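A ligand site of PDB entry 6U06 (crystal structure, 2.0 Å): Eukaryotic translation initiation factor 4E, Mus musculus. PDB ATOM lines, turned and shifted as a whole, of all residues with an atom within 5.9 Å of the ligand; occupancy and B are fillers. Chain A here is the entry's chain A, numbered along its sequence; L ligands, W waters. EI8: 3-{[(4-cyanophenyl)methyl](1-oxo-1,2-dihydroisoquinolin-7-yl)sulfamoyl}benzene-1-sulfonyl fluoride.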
ATOM      1  N   TRP A  19      25.050 -14.063 -20.003  1.00  0.00           N
ATOM      2  CA  TRP A  19      24.639 -12.803 -20.595  1.00  0.00           C
ATOM      3  C   TRP A  19      23.720 -12.072 -19.616  1.00  0.00           C
ATOM      4  O   TRP A  19      23.057 -12.698 -18.782  1.00  0.00           O
ATOM      5  CB  TRP A  19      23.909 -13.022 -21.924  1.00  0.00           C
ATOM      6  CG  TRP A  19      24.702 -13.698 -23.018  1.00  0.00           C
ATOM      7  CD1 TRP A  19      24.972 -15.037 -23.157  1.00  0.00           C
ATOM      8  CD2 TRP A  19      25.316 -13.058 -24.143  1.00  0.00           C
ATOM      9  NE1 TRP A  19      25.699 -15.253 -24.295  1.00  0.00           N
ATOM     10  CE2 TRP A  19      25.932 -14.058 -24.920  1.00  0.00           C
ATOM     11  CE3 TRP A  19      25.409 -11.733 -24.565  1.00  0.00           C
ATOM     12  CZ2 TRP A  19      26.647 -13.776 -26.091  1.00  0.00           C
ATOM     13  CZ3 TRP A  19      26.095 -11.445 -25.739  1.00  0.00           C
ATOM     14  CH2 TRP A  19      26.715 -12.471 -26.482  1.00  0.00           C
ATOM     15  N   PHE A  20      23.691 -10.738 -19.709  1.00  0.00           N
ATOM     16  CA  PHE A  20      22.800  -9.907 -18.917  1.00  0.00           C
ATOM     17  C   PHE A  20      22.122  -8.920 -19.836  1.00  0.00           C
ATOM     18  O   PHE A  20      22.726  -8.443 -20.802  1.00  0.00           O
ATOM     19  CB  PHE A  20      23.548  -9.161 -17.773  1.00  0.00           C
ATOM     20  CG  PHE A  20      22.720  -8.179 -17.000  1.00  0.00           C
ATOM     21  CD1 PHE A  20      21.924  -8.592 -15.946  1.00  0.00           C
ATOM     22  CD2 PHE A  20      22.753  -6.813 -17.304  1.00  0.00           C
ATOM     23  CE1 PHE A  20      21.163  -7.679 -15.223  1.00  0.00           C
ATOM     24  CE2 PHE A  20      21.992  -5.900 -16.580  1.00  0.00           C
ATOM     25  CZ  PHE A  20      21.197  -6.337 -15.546  1.00  0.00           C
ATOM     26  N   PHE A  21      20.868  -8.594 -19.518  1.00  0.00           N
ATOM     27  CA  PHE A  21      20.102  -7.639 -20.316  1.00  0.00           C
ATOM     28  C   PHE A  21      19.361  -6.709 -19.379  1.00  0.00           C
ATOM     29  O   PHE A  21      18.748  -7.159 -18.405  1.00  0.00           O
ATOM     30  CB  PHE A  21      19.120  -8.335 -21.273  1.00  0.00           C
ATOM     31  CG  PHE A  21      18.382  -7.383 -22.178  1.00  0.00           C
ATOM     32  CD1 PHE A  21      18.935  -6.993 -23.389  1.00  0.00           C
ATOM     33  CD2 PHE A  21      17.167  -6.804 -21.784  1.00  0.00           C
ATOM     34  CE1 PHE A  21      18.276  -6.080 -24.222  1.00  0.00           C
ATOM     35  CE2 PHE A  21      16.515  -5.871 -22.604  1.00  0.00           C
ATOM     36  CZ  PHE A  21      17.065  -5.527 -23.812  1.00  0.00           C
ATOM     37  N   TRP A  29      17.741  -2.825 -28.873  1.00  0.00           N
ATOM     38  CA  TRP A  29      17.628  -4.094 -28.145  1.00  0.00           C
ATOM     39  C   TRP A  29      18.931  -4.870 -28.227  1.00  0.00           C
ATOM     40  O   TRP A  29      19.462  -5.346 -27.215  1.00  0.00           O
ATOM     41  CB  TRP A  29      16.471  -4.929 -28.714  1.00  0.00           C
ATOM     42  CG  TRP A  29      15.952  -6.076 -27.817  1.00  0.00           C
ATOM     43  CD1 TRP A  29      14.933  -6.007 -26.893  1.00  0.00           C
ATOM     44  CD2 TRP A  29      16.406  -7.450 -27.804  1.00  0.00           C
ATOM     45  NE1 TRP A  29      14.743  -7.237 -26.297  1.00  0.00           N
ATOM     46  CE2 TRP A  29      15.629  -8.135 -26.832  1.00  0.00           C
ATOM     47  CE3 TRP A  29      17.392  -8.164 -28.503  1.00  0.00           C
ATOM     48  CZ2 TRP A  29      15.822  -9.496 -26.549  1.00  0.00           C
ATOM     49  CZ3 TRP A  29      17.570  -9.511 -28.212  1.00  0.00           C
ATOM     50  CH2 TRP A  29      16.790 -10.163 -27.244  1.00  0.00           C
ATOM     51  N   LEU A  33      22.261  -5.879 -25.018  1.00  0.00           N
ATOM     52  CA  LEU A  33      22.582  -7.225 -24.605  1.00  0.00           C
ATOM     53  C   LEU A  33      24.088  -7.331 -24.371  1.00  0.00           C
ATOM     54  O   LEU A  33      24.882  -6.746 -25.107  1.00  0.00           O
ATOM     55  CB  LEU A  33      22.095  -8.243 -25.633  1.00  0.00           C
ATOM     56  CG  LEU A  33      22.465  -9.679 -25.356  1.00  0.00           C
ATOM     57  CD1 LEU A  33      21.896 -10.190 -24.012  1.00  0.00           C
ATOM     58  CD2 LEU A  33      21.929 -10.499 -26.514  1.00  0.00           C
ATOM     59  N   ASP A  63      17.291  -9.353 -17.433  1.00  0.00           N
ATOM     60  CA  ASP A  63      17.381 -10.777 -17.709  1.00  0.00           C
ATOM     61  C   ASP A  63      18.808 -11.276 -17.481  1.00  0.00           C
ATOM     62  O   ASP A  63      19.760 -10.537 -17.657  1.00  0.00           O
ATOM     63  CB  ASP A  63      16.985 -11.079 -19.148  1.00  0.00           C
ATOM     64  CG  ASP A  63      15.740 -10.301 -19.575  1.00  0.00           C
ATOM     65  OD1 ASP A  63      14.610 -10.764 -19.335  1.00  0.00           O
ATOM     66  OD2 ASP A  63      15.893  -9.194 -20.152  1.00  0.00           O
ATOM     67  N   TYR A  64      18.923 -12.534 -17.054  1.00  0.00           N
ATOM     68  CA  TYR A  64      20.142 -13.308 -17.228  1.00  0.00           C
ATOM     69  C   TYR A  64      19.900 -14.386 -18.272  1.00  0.00           C
ATOM     70  O   TYR A  64      18.795 -14.906 -18.380  1.00  0.00           O
ATOM     71  CB  TYR A  64      20.556 -14.025 -15.949  1.00  0.00           C
ATOM     72  CG  TYR A  64      21.216 -13.221 -14.865  1.00  0.00           C
ATOM     73  CD1 TYR A  64      20.684 -13.225 -13.568  1.00  0.00           C
ATOM     74  CD2 TYR A  64      22.381 -12.517 -15.104  1.00  0.00           C
ATOM     75  CE1 TYR A  64      21.322 -12.534 -12.547  1.00  0.00           C
ATOM     76  CE2 TYR A  64      23.019 -11.826 -14.083  1.00  0.00           C
ATOM     77  CZ  TYR A  64      22.478 -11.833 -12.809  1.00  0.00           C
ATOM     78  OH  TYR A  64      23.116 -11.134 -11.793  1.00  0.00           O
ATOM     79  N   SER A  65      20.939 -14.764 -19.012  1.00  0.00           N
ATOM     80  CA  SER A  65      20.825 -16.003 -19.750  1.00  0.00           C
ATOM     81  C   SER A  65      22.157 -16.732 -19.762  1.00  0.00           C
ATOM     82  O   SER A  65      23.230 -16.135 -19.618  1.00  0.00           O
ATOM     83  CB  SER A  65      20.302 -15.762 -21.183  1.00  0.00           C
ATOM     84  OG  SER A  65      21.238 -15.009 -21.907  1.00  0.00           O
ATOM     85  N   PRO A  73      21.815 -15.453 -27.217  1.00  0.00           N
ATOM     86  CA  PRO A  73      20.513 -15.683 -26.563  1.00  0.00           C
ATOM     87  C   PRO A  73      19.395 -14.911 -27.237  1.00  0.00           C
ATOM     88  O   PRO A  73      18.751 -14.041 -26.629  1.00  0.00           O
ATOM     89  CB  PRO A  73      20.773 -15.224 -25.128  1.00  0.00           C
ATOM     90  CG  PRO A  73      21.745 -14.120 -25.271  1.00  0.00           C
ATOM     91  CD  PRO A  73      22.650 -14.512 -26.427  1.00  0.00           C
ATOM     92  N   MET A  74      19.172 -15.195 -28.513  1.00  0.00           N
ATOM     93  CA  MET A  74      18.053 -14.594 -29.215  1.00  0.00           C
ATOM     94  C   MET A  74      17.565 -15.564 -30.281  1.00  0.00           C
ATOM     95  O   MET A  74      18.334 -16.401 -30.786  1.00  0.00           O
ATOM     96  CB  MET A  74      18.400 -13.211 -29.807  1.00  0.00           C
ATOM     97  CG  MET A  74      19.695 -13.147 -30.575  1.00  0.00           C
ATOM     98  SD  MET A  74      20.228 -11.451 -30.930  1.00  0.00           S
ATOM     99  CE  MET A  74      18.723 -10.703 -31.561  1.00  0.00           C
ATOM    100  N   TRP A  75      16.286 -15.436 -30.622  1.00  0.00           N
ATOM    101  CA  TRP A  75      15.645 -16.353 -31.569  1.00  0.00           C
ATOM    102  C   TRP A  75      16.361 -16.364 -32.909  1.00  0.00           C
ATOM    103  O   TRP A  75      16.312 -17.368 -33.626  1.00  0.00           O
ATOM    104  CB  TRP A  75      14.190 -15.958 -31.824  1.00  0.00           C
ATOM    105  CG  TRP A  75      13.383 -15.817 -30.598  1.00  0.00           C
ATOM    106  CD1 TRP A  75      13.537 -16.496 -29.432  1.00  0.00           C
ATOM    107  CD2 TRP A  75      12.276 -14.932 -30.402  1.00  0.00           C
ATOM    108  NE1 TRP A  75      12.593 -16.096 -28.522  1.00  0.00           N
ATOM    109  CE2 TRP A  75      11.805 -15.129 -29.087  1.00  0.00           C
ATOM    110  CE3 TRP A  75      11.644 -13.978 -31.211  1.00  0.00           C
ATOM    111  CZ2 TRP A  75      10.737 -14.427 -28.563  1.00  0.00           C
ATOM    112  CZ3 TRP A  75      10.583 -13.278 -30.693  1.00  0.00           C
ATOM    113  CH2 TRP A  75      10.135 -13.501 -29.387  1.00  0.00           C
ATOM    114  N   GLU A  76      16.981 -15.246 -33.282  1.00  0.00           N
ATOM    115  CA  GLU A  76      17.554 -15.089 -34.607  1.00  0.00           C
ATOM    116  C   GLU A  76      18.754 -16.009 -34.840  1.00  0.00           C
ATOM    117  O   GLU A  76      19.095 -16.294 -35.989  1.00  0.00           O
ATOM    118  CB  GLU A  76      17.934 -13.623 -34.802  1.00  0.00           C
ATOM    119  CG  GLU A  76      16.741 -12.673 -34.962  1.00  0.00           C
ATOM    120  CD  GLU A  76      15.995 -12.359 -33.660  1.00  0.00           C
ATOM    121  OE1 GLU A  76      16.191 -13.062 -32.637  1.00  0.00           O
ATOM    122  OE2 GLU A  76      15.174 -11.407 -33.667  1.00  0.00           O
ATOM    123  N   ARG A  85      11.156 -23.427 -26.278  1.00  0.00           N
ATOM    124  CA  ARG A  85      11.541 -23.346 -24.869  1.00  0.00           C
ATOM    125  C   ARG A  85      10.520 -24.079 -23.998  1.00  0.00           C
ATOM    126  O   ARG A  85       9.328 -24.109 -24.309  1.00  0.00           O
ATOM    127  CB  ARG A  85      11.676 -21.899 -24.393  1.00  0.00           C
ATOM    128  CG  ARG A  85      10.346 -21.164 -24.335  1.00  0.00           C
ATOM    129  CD  ARG A  85      10.537 -19.685 -24.029  1.00  0.00           C
ATOM    130  NE  ARG A  85       9.276 -18.965 -24.029  1.00  0.00           N
ATOM    131  CZ  ARG A  85       9.149 -17.674 -23.729  1.00  0.00           C
ATOM    132  NH1 ARG A  85       7.949 -17.091 -23.753  1.00  0.00           N
ATOM    133  NH2 ARG A  85      10.218 -16.963 -23.381  1.00  0.00           N
ATOM    134  N   VAL A 126      17.114 -18.842 -19.953  1.00  0.00           N
ATOM    135  CA  VAL A 126      16.853 -17.414 -19.786  1.00  0.00           C
ATOM    136  C   VAL A 126      15.986 -17.222 -18.541  1.00  0.00           C
ATOM    137  O   VAL A 126      14.987 -17.916 -18.359  1.00  0.00           O
ATOM    138  CB  VAL A 126      16.139 -16.808 -21.009  1.00  0.00           C
ATOM    139  CG1 VAL A 126      15.700 -15.363 -20.718  1.00  0.00           C
ATOM    140  CG2 VAL A 126      17.010 -16.900 -22.283  1.00  0.00           C
ATOM    141  N   ASN A 128      13.743 -14.096 -16.942  1.00  0.00           N
ATOM    142  CA  ASN A 128      13.196 -12.745 -17.107  1.00  0.00           C
ATOM    143  C   ASN A 128      12.622 -12.278 -15.785  1.00  0.00           C
ATOM    144  O   ASN A 128      11.689 -12.903 -15.257  1.00  0.00           O
ATOM    145  CB  ASN A 128      12.115 -12.682 -18.191  1.00  0.00           C
ATOM    146  CG  ASN A 128      12.460 -13.522 -19.396  1.00  0.00           C
ATOM    147  OD1 ASN A 128      11.913 -14.612 -19.589  1.00  0.00           O
ATOM    148  ND2 ASN A 128      13.345 -13.000 -20.235  1.00  0.00           N
ATOM    149  N   ARG A 130      10.372  -9.577 -14.240  1.00  0.00           N
ATOM    150  CA  ARG A 130       9.325  -8.687 -14.739  1.00  0.00           C
ATOM    151  C   ARG A 130       8.372  -8.342 -13.612  1.00  0.00           C
ATOM    152  O   ARG A 130       8.122  -9.161 -12.720  1.00  0.00           O
ATOM    153  CB  ARG A 130       8.532  -9.341 -15.897  1.00  0.00           C
ATOM    154  CG  ARG A 130       9.364  -9.681 -17.125  1.00  0.00           C
ATOM    155  CD  ARG A 130       9.795  -8.434 -17.918  1.00  0.00           C
ATOM    156  NE  ARG A 130      10.485  -8.848 -19.140  1.00  0.00           N
ATOM    157  CZ  ARG A 130      11.766  -9.217 -19.207  1.00  0.00           C
ATOM    158  NH1 ARG A 130      12.544  -9.217 -18.109  1.00  0.00           N
ATOM    159  NH2 ARG A 130      12.265  -9.599 -20.356  1.00  0.00           N
ATOM    160  N   LYS A 132       5.107  -7.926 -13.770  1.00  0.00           N
ATOM    161  CA  LYS A 132       3.914  -8.758 -13.809  1.00  0.00           C
ATOM    162  C   LYS A 132       4.190 -10.229 -13.492  1.00  0.00           C
ATOM    163  O   LYS A 132       3.237 -11.005 -13.377  1.00  0.00           O
ATOM    164  CB  LYS A 132       3.222  -8.642 -15.178  1.00  0.00           C
ATOM    165  CG  LYS A 132       4.070  -9.084 -16.402  1.00  0.00           C
ATOM    166  CD  LYS A 132       3.901 -10.555 -16.796  1.00  0.00           C
ATOM    167  CE  LYS A 132       5.192 -11.143 -17.335  1.00  0.00           C
ATOM    168  NZ  LYS A 132       5.156 -12.629 -17.455  1.00  0.00           N
ATOM    169  N   GLY A 133       5.444 -10.636 -13.386  1.00  0.00           N
ATOM    170  CA  GLY A 133       5.726 -12.016 -13.076  1.00  0.00           C
ATOM    171  C   GLY A 133       6.974 -12.540 -13.754  1.00  0.00           C
ATOM    172  O   GLY A 133       7.179 -12.309 -14.955  1.00  0.00           O
ATOM    173  N   LYS A 135       9.889 -15.321 -15.149  1.00  0.00           N
ATOM    174  CA  LYS A 135       9.841 -16.494 -15.986  1.00  0.00           C
ATOM    175  C   LYS A 135      11.241 -17.089 -16.081  1.00  0.00           C
ATOM    176  O   LYS A 135      12.233 -16.371 -16.127  1.00  0.00           O
ATOM    177  CB  LYS A 135       9.353 -16.167 -17.421  1.00  0.00           C
ATOM    178  CG  LYS A 135       7.921 -15.662 -17.503  1.00  0.00           C
ATOM    179  CD  LYS A 135       7.473 -15.628 -18.942  1.00  0.00           C
ATOM    180  CE  LYS A 135       7.227 -14.214 -19.414  1.00  0.00           C
ATOM    181  NZ  LYS A 135       8.479 -13.546 -19.790  1.00  0.00           N
ATOM    182  N   TRP A 139      15.917 -23.228 -23.431  1.00  0.00           N
ATOM    183  CA  TRP A 139      15.808 -23.171 -24.887  1.00  0.00           C
ATOM    184  C   TRP A 139      16.511 -24.379 -25.502  1.00  0.00           C
ATOM    185  O   TRP A 139      17.639 -24.696 -25.127  1.00  0.00           O
ATOM    186  CB  TRP A 139      16.466 -21.902 -25.445  1.00  0.00           C
ATOM    187  CG  TRP A 139      15.757 -20.605 -25.126  1.00  0.00           C
ATOM    188  CD1 TRP A 139      14.907 -20.353 -24.076  1.00  0.00           C
ATOM    189  CD2 TRP A 139      15.837 -19.382 -25.883  1.00  0.00           C
ATOM    190  NE1 TRP A 139      14.457 -19.043 -24.117  1.00  0.00           N
ATOM    191  CE2 TRP A 139      15.018 -18.433 -25.223  1.00  0.00           C
ATOM    192  CE3 TRP A 139      16.522 -19.001 -27.040  1.00  0.00           C
ATOM    193  CZ2 TRP A 139      14.874 -17.129 -25.703  1.00  0.00           C
ATOM    194  CZ3 TRP A 139      16.380 -17.706 -27.498  1.00  0.00           C
ATOM    195  CH2 TRP A 139      15.551 -16.783 -26.822  1.00  0.00           C
ATOM    196  N   HIS A 173       9.775 -20.994 -30.645  1.00  0.00           N
ATOM    197  CA  HIS A 173      10.091 -19.577 -30.793  1.00  0.00           C
ATOM    198  C   HIS A 173       9.283 -18.953 -31.927  1.00  0.00           C
ATOM    199  O   HIS A 173       8.705 -17.877 -31.763  1.00  0.00           O
ATOM    200  CB  HIS A 173      11.589 -19.394 -31.029  1.00  0.00           C
ATOM    201  CG  HIS A 173      12.444 -19.814 -29.880  1.00  0.00           C
ATOM    202  ND1 HIS A 173      12.089 -19.573 -28.570  1.00  0.00           N
ATOM    203  CD2 HIS A 173      13.637 -20.457 -29.836  1.00  0.00           C
ATOM    204  CE1 HIS A 173      13.026 -20.054 -27.767  1.00  0.00           C
ATOM    205  NE2 HIS A 173      13.979 -20.587 -28.511  1.00  0.00           N
ATOM    206  N   THR A 176       6.014 -18.229 -30.646  1.00  0.00           N
ATOM    207  CA  THR A 176       6.098 -17.162 -29.643  1.00  0.00           C
ATOM    208  C   THR A 176       6.207 -15.792 -30.283  1.00  0.00           C
ATOM    209  O   THR A 176       5.691 -14.801 -29.735  1.00  0.00           O
ATOM    210  CB  THR A 176       7.292 -17.422 -28.730  1.00  0.00           C
ATOM    211  OG1 THR A 176       7.067 -18.609 -27.961  1.00  0.00           O
ATOM    212  CG2 THR A 176       7.539 -16.242 -27.791  1.00  0.00           C
HETATM  213  C1  EI8 L   1      18.818 -12.265 -22.864  1.00  0.00           C
HETATM  214  C10 EI8 L   1      12.573 -11.137 -28.645  1.00  0.00           C
HETATM  215  C11 EI8 L   1      12.531 -10.600 -29.932  1.00  0.00           C
HETATM  216  C12 EI8 L   1      13.390 -11.060 -30.920  1.00  0.00           C
HETATM  217  C13 EI8 L   1      14.378 -12.619 -29.442  1.00  0.00           C
HETATM  218  C14 EI8 L   1      13.469 -12.155 -28.341  1.00  0.00           C
HETATM  219  C15 EI8 L   1      13.533 -12.701 -27.056  1.00  0.00           C
HETATM  220  C16 EI8 L   1      10.445 -13.592 -23.888  1.00  0.00           C
HETATM  221  C17 EI8 L   1      10.128 -13.158 -22.599  1.00  0.00           C
HETATM  222  C18 EI8 L   1       8.832 -12.742 -22.261  1.00  0.00           C
HETATM  223  C19 EI8 L   1       7.832 -12.790 -23.235  1.00  0.00           C
HETATM  224  C2  EI8 L   1      17.557 -12.180 -23.087  1.00  0.00           C
HETATM  225  C20 EI8 L   1       8.148 -13.216 -24.530  1.00  0.00           C
HETATM  226  C21 EI8 L   1       9.442 -13.599 -24.855  1.00  0.00           C
HETATM  227  C22 EI8 L   1      15.459 -11.025 -22.758  1.00  0.00           C
HETATM  228  C23 EI8 L   1      16.827 -11.113 -22.542  1.00  0.00           C
HETATM  229  C3  EI8 L   1      16.906 -13.153 -23.834  1.00  0.00           C
HETATM  230  C4  EI8 L   1      15.537 -13.049 -24.043  1.00  0.00           C
HETATM  231  C5  EI8 L   1      14.800 -11.993 -23.515  1.00  0.00           C
HETATM  232  C6  EI8 L   1      13.295 -11.872 -23.725  1.00  0.00           C
HETATM  233  C7  EI8 L   1      12.662 -12.251 -26.062  1.00  0.00           C
HETATM  234  C8  EI8 L   1      11.765 -11.224 -26.371  1.00  0.00           C
HETATM  235  C9  EI8 L   1      11.708 -10.673 -27.651  1.00  0.00           C
HETATM  236  N1  EI8 L   1      19.932 -12.354 -22.595  1.00  0.00           N
HETATM  237  N2  EI8 L   1      12.666 -12.732 -24.734  1.00  0.00           N
HETATM  238  N3  EI8 L   1      14.279 -12.043 -30.671  1.00  0.00           N
HETATM  239  O1  EI8 L   1      15.214 -13.529 -29.237  1.00  0.00           O
HETATM  240  O2  EI8 L   1      11.906 -15.031 -25.308  1.00  0.00           O
HETATM  241  O3  EI8 L   1      12.640 -14.570 -23.147  1.00  0.00           O
HETATM  242  O4  EI8 L   1       9.363 -11.310 -20.225  1.00  0.00           O
HETATM  243  O5  EI8 L   1       7.146 -11.716 -20.734  1.00  0.00           O
HETATM  244  S1  EI8 L   1      11.953 -14.026 -24.283  1.00  0.00           S
HETATM  245  S2  EI8 L   1       8.463 -12.281 -20.763  1.00  0.00           S
HETATM  246  O   HOH W   1       8.659  -8.305 -21.452  1.00  0.00           O
HETATM  247  O   HOH W   2      12.756 -17.425 -22.548  1.00  0.00           O
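An oxygen (O3) of the ligand is in hydrogen-bond range of the side-chain amide nitrogen of Asn 128, at 3.4 Å.
An oxygen (O2) of the ligand sits at hydrogen-bond distance from the indole nitrogen (NE1) of Trp 75 (3.5 Å).
The side-chain carboxylate of Glu 76 sits at hydrogen-bond distance from a nitrogen (N3) of the ligand (2.9 Å).
NE of Arg 130 sits at hydrogen-bond distance from O4 of the ligand.
NZ of Lys 135 is covalently linked to S2 of the ligand, at 1.6 Å.
An oxygen (O2) of the ligand is in hydrogen-bond range of the guanidinium group (NH2) of Arg 85.
The side-chain hydroxyl (OG) of Ser 65 lies within hydrogen-bond range of a nitrogen (N1) of the ligand (3.0 Å).
N of Trp 75 is in hydrogen-bond range of O1 of the ligand (2.6 Å).
The side-chain amide nitrogen of Asn 128 lies within hydrogen-bond range of the side-chain carboxylate of Asp 63, 2.7 Å away.
O of Phe 21 sits at hydrogen-bond distance from N of Asp 63, at 2.8 Å.
N of Asn 128 lies within hydrogen-bond range of O of Lys 135, at 2.8 Å.
The backbone carbonyl oxygen of Ser 65 sits at hydrogen-bond distance from the backbone NH of Trp 19, at 2.8 Å.
OD1 of Asp 63 is in salt-bridge range of NH2 of Arg 130.
Merely in contact with the ligand: Phe 21 (3.8 Å), Trp 29 (3.97 Å), Leu 33 (3.2 Å), Asp 63 (3.2 Å), Pro 73 (3.5 Å), Met 74 (3.0 Å), Val 126 (3.99 Å), Lys 132 (3.9 Å) and Trp 139 (3.7 Å).
Hydrophobic or aromatic side chains that line the ligand: Phe 21, Trp 29, Leu 33, Pro 73, Met 74, Trp 75, Val 126 and Trp 139.
Within 4 Å of the ligand: Phe 21, Trp 29, Leu 33, Asp 63, Ser 65, Pro 73, Met 74, Trp 75, Glu 76, Arg 85, Val 126, Asn 128, Arg 130, Lys 132, Lys 135 and Trp 139.
The nearest printed residue that does not touch the ligand is Trp 19 (4.1 Å).
Water W2 lies within hydrogen-bond range of NH2 of Arg 85 (2.7 Å), NE1 of Trp 139 (2.8 Å) and O3 of the ligand (2.9 Å).
Water W1 lies within hydrogen-bond range of the guanidinium group of Arg 130 and an oxygen (O4) of the ligand.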
